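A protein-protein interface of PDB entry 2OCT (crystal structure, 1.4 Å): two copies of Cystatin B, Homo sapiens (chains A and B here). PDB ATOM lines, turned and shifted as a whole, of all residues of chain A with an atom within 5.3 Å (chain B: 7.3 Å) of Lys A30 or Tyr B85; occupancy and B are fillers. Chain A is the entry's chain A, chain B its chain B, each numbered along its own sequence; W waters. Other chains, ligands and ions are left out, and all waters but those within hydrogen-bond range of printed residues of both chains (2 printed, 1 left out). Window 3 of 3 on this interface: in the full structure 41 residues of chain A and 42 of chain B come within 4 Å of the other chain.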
ATOM      1  N   GLN A  26      20.781  -3.518  24.569  1.00  0.00           N
ATOM      2  CA  GLN A  26      21.225  -2.766  25.738  1.00  0.00           C
ATOM      3  C   GLN A  26      20.206  -2.911  26.858  1.00  0.00           C
ATOM      4  O   GLN A  26      20.528  -3.159  28.021  1.00  0.00           O
ATOM      5  CB  GLN A  26      21.408  -1.299  25.338  1.00  0.00           C
ATOM      6  CG  GLN A  26      22.266  -0.505  26.291  1.00  0.00           C
ATOM      7  CD  GLN A  26      22.173   0.988  25.937  1.00  0.00           C
ATOM      8  OE1 GLN A  26      22.278   1.871  26.790  1.00  0.00           O
ATOM      9  NE2 GLN A  26      21.963   1.228  24.643  1.00  0.00           N
ATOM     10  N   LEU A  27      18.924  -2.779  26.544  1.00  0.00           N
ATOM     11  CA  LEU A  27      17.897  -2.861  27.574  1.00  0.00           C
ATOM     12  C   LEU A  27      17.790  -4.259  28.180  1.00  0.00           C
ATOM     13  O   LEU A  27      17.639  -4.343  29.410  1.00  0.00           O
ATOM     14  CB  LEU A  27      16.530  -2.447  27.021  1.00  0.00           C
ATOM     15  CG  LEU A  27      15.422  -2.318  28.078  1.00  0.00           C
ATOM     16  CD1 LEU A  27      15.841  -1.384  29.203  1.00  0.00           C
ATOM     17  CD2 LEU A  27      14.136  -1.833  27.425  1.00  0.00           C
ATOM     18  N   GLU A  28      17.867  -5.263  27.321  1.00  0.00           N
ATOM     19  CA  GLU A  28      17.834  -6.673  27.682  1.00  0.00           C
ATOM     20  C   GLU A  28      18.965  -7.010  28.643  1.00  0.00           C
ATOM     21  O   GLU A  28      18.890  -7.971  29.422  1.00  0.00           O
ATOM     22  CB  GLU A  28      17.913  -7.557  26.429  1.00  0.00           C
ATOM     23  CG  GLU A  28      16.634  -7.585  25.611  1.00  0.00           C
ATOM     24  CD  GLU A  28      16.666  -8.480  24.406  1.00  0.00           C
ATOM     25  OE1 GLU A  28      17.780  -8.768  23.934  1.00  0.00           O
ATOM     26  OE2 GLU A  28      15.620  -8.923  23.872  1.00  0.00           O
ATOM     27  N   GLU A  29      20.048  -6.225  28.619  1.00  0.00           N
ATOM     28  CA  GLU A  29      21.089  -6.462  29.643  1.00  0.00           C
ATOM     29  C   GLU A  29      20.548  -6.131  31.035  1.00  0.00           C
ATOM     30  O   GLU A  29      20.782  -6.794  32.053  1.00  0.00           O
ATOM     31  CB  GLU A  29      22.349  -5.663  29.330  1.00  0.00           C
ATOM     32  CG  GLU A  29      23.203  -5.238  30.524  1.00  0.00           C
ATOM     33  CD  GLU A  29      24.609  -4.801  30.146  1.00  0.00           C
ATOM     34  OE1 GLU A  29      24.883  -4.772  28.923  1.00  0.00           O
ATOM     35  OE2 GLU A  29      25.462  -4.486  31.013  1.00  0.00           O
ATOM     36  N   LYS A  30      19.791  -5.033  31.052  1.00  0.00           N
ATOM     37  CA  LYS A  30      19.190  -4.507  32.259  1.00  0.00           C
ATOM     38  C   LYS A  30      18.416  -5.610  32.970  1.00  0.00           C
ATOM     39  O   LYS A  30      18.722  -5.853  34.131  1.00  0.00           O
ATOM     40  CB  LYS A  30      18.254  -3.340  31.948  1.00  0.00           C
ATOM     41  CG  LYS A  30      18.968  -2.095  31.456  1.00  0.00           C
ATOM     42  CD  LYS A  30      20.464  -2.188  31.714  1.00  0.00           C
ATOM     43  CE  LYS A  30      21.239  -1.458  30.632  1.00  0.00           C
ATOM     44  NZ  LYS A  30      22.193  -2.343  29.898  1.00  0.00           N
ATOM     45  N   TYR A  31      17.463  -6.229  32.283  1.00  0.00           N
ATOM     46  CA  TYR A  31      16.564  -7.176  32.910  1.00  0.00           C
ATOM     47  C   TYR A  31      17.193  -8.570  32.977  1.00  0.00           C
ATOM     48  O   TYR A  31      16.536  -9.490  33.470  1.00  0.00           O
ATOM     49  CB  TYR A  31      15.252  -7.362  32.166  1.00  0.00           C
ATOM     50  CG  TYR A  31      14.251  -6.278  31.949  1.00  0.00           C
ATOM     51  CD1 TYR A  31      14.587  -5.000  31.509  1.00  0.00           C
ATOM     52  CD2 TYR A  31      12.906  -6.564  32.190  1.00  0.00           C
ATOM     53  CE1 TYR A  31      13.606  -4.042  31.324  1.00  0.00           C
ATOM     54  CE2 TYR A  31      11.922  -5.616  32.010  1.00  0.00           C
ATOM     55  CZ  TYR A  31      12.289  -4.359  31.575  1.00  0.00           C
ATOM     56  OH  TYR A  31      11.303  -3.420  31.400  1.00  0.00           O
ATOM     57  N   ASN A  32      18.409  -8.740  32.474  1.00  0.00           N
ATOM     58  CA  ASN A  32      19.055 -10.060  32.593  1.00  0.00           C
ATOM     59  C   ASN A  32      18.349 -11.099  31.737  1.00  0.00           C
ATOM     60  O   ASN A  32      18.671 -12.291  31.872  1.00  0.00           O
ATOM     61  CB  ASN A  32      19.087 -10.474  34.056  1.00  0.00           C
ATOM     62  CG  ASN A  32      20.115 -11.430  34.582  1.00  0.00           C
ATOM     63  OD1 ASN A  32      21.330 -11.179  34.586  1.00  0.00           O
ATOM     64  ND2 ASN A  32      19.666 -12.580  35.099  1.00  0.00           N
ATOM     65  N   VAL B  65       7.309  -1.485  27.817  1.00  0.00           N
ATOM     66  CA  VAL B  65       8.286  -0.569  28.383  1.00  0.00           C
ATOM     67  C   VAL B  65       8.164   0.729  27.615  1.00  0.00           C
ATOM     68  O   VAL B  65       7.707   0.736  26.461  1.00  0.00           O
ATOM     69  CB  VAL B  65       9.723  -1.088  28.303  1.00  0.00           C
ATOM     70  CG1 VAL B  65       9.782  -2.405  29.065  1.00  0.00           C
ATOM     71  CG2 VAL B  65      10.235  -1.302  26.882  1.00  0.00           C
ATOM     72  N   HIS B  66       8.594   1.824  28.215  1.00  0.00           N
ATOM     73  CA  HIS B  66       8.683   3.071  27.480  1.00  0.00           C
ATOM     74  C   HIS B  66      10.142   3.471  27.352  1.00  0.00           C
ATOM     75  O   HIS B  66      10.920   3.424  28.294  1.00  0.00           O
ATOM     76  CB  HIS B  66       7.922   4.184  28.188  1.00  0.00           C
ATOM     77  CG  HIS B  66       6.432   4.114  28.095  1.00  0.00           C
ATOM     78  ND1 HIS B  66       5.690   3.069  27.621  1.00  0.00           N
ATOM     79  CD2 HIS B  66       5.536   5.073  28.464  1.00  0.00           C
ATOM     80  CE1 HIS B  66       4.396   3.339  27.680  1.00  0.00           C
ATOM     81  NE2 HIS B  66       4.291   4.554  28.191  1.00  0.00           N
ATOM     82  N   LEU B  67      10.562   3.874  26.173  1.00  0.00           N
ATOM     83  CA  LEU B  67      11.938   4.241  25.948  1.00  0.00           C
ATOM     84  C   LEU B  67      12.106   5.734  25.716  1.00  0.00           C
ATOM     85  O   LEU B  67      11.202   6.320  25.090  1.00  0.00           O
ATOM     86  CB  LEU B  67      12.498   3.591  24.666  1.00  0.00           C
ATOM     87  CG  LEU B  67      12.261   2.084  24.583  1.00  0.00           C
ATOM     88  CD1 LEU B  67      12.774   1.563  23.247  1.00  0.00           C
ATOM     89  CD2 LEU B  67      12.879   1.369  25.771  1.00  0.00           C
ATOM     90  N   ARG B  68      13.206   6.310  26.179  1.00  0.00           N
ATOM     91  CA  ARG B  68      13.577   7.662  25.746  1.00  0.00           C
ATOM     92  C   ARG B  68      14.866   7.545  24.950  1.00  0.00           C
ATOM     93  O   ARG B  68      15.895   7.150  25.546  1.00  0.00           O
ATOM     94  CB  ARG B  68      13.781   8.571  26.960  1.00  0.00           C
ATOM     95  CG  ARG B  68      14.473   9.874  26.615  1.00  0.00           C
ATOM     96  CD  ARG B  68      14.747  10.680  27.908  1.00  0.00           C
ATOM     97  NE  ARG B  68      15.526  11.864  27.591  1.00  0.00           N
ATOM     98  CZ  ARG B  68      15.475  13.056  28.175  1.00  0.00           C
ATOM     99  NH1 ARG B  68      14.609  13.244  29.161  1.00  0.00           N
ATOM    100  NH2 ARG B  68      16.277  14.045  27.757  1.00  0.00           N
ATOM    101  N   LEU B  82      20.157   5.393  23.882  1.00  0.00           N
ATOM    102  CA  LEU B  82      19.128   5.113  24.882  1.00  0.00           C
ATOM    103  C   LEU B  82      19.385   5.948  26.139  1.00  0.00           C
ATOM    104  O   LEU B  82      20.293   5.615  26.928  1.00  0.00           O
ATOM    105  CB  LEU B  82      19.100   3.623  25.253  1.00  0.00           C
ATOM    106  CG  LEU B  82      17.997   3.192  26.207  1.00  0.00           C
ATOM    107  CD1 LEU B  82      16.616   3.467  25.631  1.00  0.00           C
ATOM    108  CD2 LEU B  82      18.105   1.698  26.529  1.00  0.00           C
ATOM    109  N   SER B  83      18.623   7.003  26.373  1.00  0.00           N
ATOM    110  CA  SER B  83      18.890   7.915  27.484  1.00  0.00           C
ATOM    111  C   SER B  83      18.259   7.407  28.777  1.00  0.00           C
ATOM    112  O   SER B  83      18.749   7.606  29.883  1.00  0.00           O
ATOM    113  CB  SER B  83      18.314   9.309  27.225  1.00  0.00           C
ATOM    114  OG  SER B  83      18.982  10.008  26.205  1.00  0.00           O
ATOM    115  N   ASN B  84      17.090   6.771  28.671  1.00  0.00           N
ATOM    116  CA  ASN B  84      16.431   6.270  29.892  1.00  0.00           C
ATOM    117  C   ASN B  84      15.357   5.297  29.426  1.00  0.00           C
ATOM    118  O   ASN B  84      15.207   5.116  28.210  1.00  0.00           O
ATOM    119  CB  ASN B  84      15.878   7.429  30.694  1.00  0.00           C
ATOM    120  CG  ASN B  84      15.682   7.202  32.179  1.00  0.00           C
ATOM    121  OD1 ASN B  84      15.765   6.079  32.651  1.00  0.00           O
ATOM    122  ND2 ASN B  84      15.443   8.294  32.933  1.00  0.00           N
ATOM    123  N   TYR B  85      14.637   4.718  30.364  1.00  0.00           N
ATOM    124  CA  TYR B  85      13.499   3.839  30.096  1.00  0.00           C
ATOM    125  C   TYR B  85      12.647   3.693  31.345  1.00  0.00           C
ATOM    126  O   TYR B  85      13.134   3.926  32.457  1.00  0.00           O
ATOM    127  CB  TYR B  85      13.920   2.448  29.604  1.00  0.00           C
ATOM    128  CG  TYR B  85      14.766   1.642  30.559  1.00  0.00           C
ATOM    129  CD1 TYR B  85      16.151   1.729  30.529  1.00  0.00           C
ATOM    130  CD2 TYR B  85      14.188   0.785  31.492  1.00  0.00           C
ATOM    131  CE1 TYR B  85      16.936   0.994  31.400  1.00  0.00           C
ATOM    132  CE2 TYR B  85      14.963   0.056  32.362  1.00  0.00           C
ATOM    133  CZ  TYR B  85      16.338   0.160  32.317  1.00  0.00           C
ATOM    134  OH  TYR B  85      17.126  -0.576  33.178  1.00  0.00           O
ATOM    135  N   GLN B  86      11.407   3.266  31.138  1.00  0.00           N
ATOM    136  CA  GLN B  86      10.524   2.877  32.243  1.00  0.00           C
ATOM    137  C   GLN B  86      10.102   1.422  32.077  1.00  0.00           C
ATOM    138  O   GLN B  86       9.699   1.062  30.960  1.00  0.00           O
ATOM    139  CB  GLN B  86       9.326   3.824  32.287  1.00  0.00           C
ATOM    140  CG  GLN B  86       9.783   5.264  32.605  1.00  0.00           C
ATOM    141  CD  GLN B  86       8.616   6.217  32.701  1.00  0.00           C
ATOM    142  OE1 GLN B  86       7.567   5.953  32.112  1.00  0.00           O
ATOM    143  NE2 GLN B  86       8.787   7.306  33.442  1.00  0.00           N
ATOM    144  N   THR B  87      10.222   0.668  33.149  1.00  0.00           N
ATOM    145  CA  THR B  87       9.831  -0.700  33.385  1.00  0.00           C
ATOM    146  C   THR B  87       8.325  -0.799  33.694  1.00  0.00           C
ATOM    147  O   THR B  87       7.670   0.165  34.071  1.00  0.00           O
ATOM    148  CB  THR B  87      10.446  -1.450  34.600  1.00  0.00           C
ATOM    149  OG1 THR B  87      10.474  -0.575  35.740  1.00  0.00           O
ATOM    150  CG2 THR B  87      11.870  -1.912  34.369  1.00  0.00           C
ATOM    151  N   ASN B  88       7.865  -2.045  33.538  1.00  0.00           N
ATOM    152  CA  ASN B  88       6.531  -2.427  33.965  1.00  0.00           C
ATOM    153  C   ASN B  88       5.446  -1.449  33.560  1.00  0.00           C
ATOM    154  O   ASN B  88       4.631  -1.040  34.379  1.00  0.00           O
ATOM    155  CB  ASN B  88       6.498  -2.571  35.506  1.00  0.00           C
ATOM    156  CG  ASN B  88       6.272  -4.036  35.828  1.00  0.00           C
ATOM    157  OD1 ASN B  88       7.046  -4.615  36.588  1.00  0.00           O
ATOM    158  ND2 ASN B  88       5.229  -4.617  35.236  1.00  0.00           N
ATOM    159  N   PHE B  98       9.966  11.851  30.494  1.00  0.00           N
ATOM    160  CA  PHE B  98      10.739  11.453  31.673  1.00  0.00           C
ATOM    161  C   PHE B  98      12.221  11.577  31.290  1.00  0.00           C
ATOM    162  O   PHE B  98      12.391  11.738  30.052  1.00  0.00           O
ATOM    163  CB  PHE B  98      10.427  10.038  32.152  1.00  0.00           C
ATOM    164  CG  PHE B  98      10.604   8.984  31.052  1.00  0.00           C
ATOM    165  CD1 PHE B  98       9.602   8.747  30.125  1.00  0.00           C
ATOM    166  CD2 PHE B  98      11.765   8.245  30.955  1.00  0.00           C
ATOM    167  CE1 PHE B  98       9.773   7.802  29.132  1.00  0.00           C
ATOM    168  CE2 PHE B  98      11.936   7.298  29.950  1.00  0.00           C
ATOM    169  CZ  PHE B  98      10.939   7.057  29.014  1.00  0.00           C
ATOM    170  OXT PHE B  98      13.040  11.529  32.105  1.00  0.00           O
HETATM  171  O   HOH W   1      23.268   4.787  26.370  1.00  0.00           O
HETATM  172  O   HOH W   2      22.261   3.463  23.575  1.00  0.00           O
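Lys A30 touches one residue of chain B. Tyr B85 touches just these residues of chain A: Leu A27 and Lys A30. Of the printed residues of chain A, Leu B82 touches Gln A26 (3.8 Å). Printed residues of chain B within 4 Å of Leu A27: Val B65 (3.97 Å), Leu B67 (3.8 Å) and Tyr B85 (3.4 Å). The nearest residue of chain B that does not touch Lys A30 is Leu B82 (6.1 Å).
Of the 12 printed residues of chain B, 5 touch a printed residue of chain A. Printed residues of chain B that touch a printed residue of chain A: Val B65, Leu B67, Leu B82, Tyr B85 and Thr B87. Of the 7 printed residues of chain A, 4 touch a printed residue of chain B. Printed residues of chain A that touch a printed residue of chain B: Gln A26, Leu A27, Lys A30 and Tyr A31. Among the printed residues, 7 pairs touch across the chains.
The side-chain amino group of Lys A30 is in hydrogen-bond range of the backbone carbonyl oxygen of Gln A26 (2.6 Å). The side-chain carboxylate (OE1) of Glu A29 lies within salt-bridge range of the side-chain amino group (NZ) of Lys A30 (3.8 Å).
Water W2 lies within hydrogen-bond range of NE2 of Gln A26 (2.5 Å) and N of Leu B82 (2.9 Å). Water W1 bridges OE1 of Gln A26 and O of Leu B82.
Among the printed residues, pairs that only touch across the chains: Gln A26 with Leu B82 (3.8 Å), Leu A27 with Val B65 (3.97 Å), Leu A27 with Leu B67 (3.8 Å), Leu A27 with Tyr B85 (3.4 Å), Lys A30 with Tyr B85 (2.9 Å), Tyr A31 with Val B65 (3.0 Å) and Tyr A31 with Thr B87 (3.4 Å).
No position is printed for both chains.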
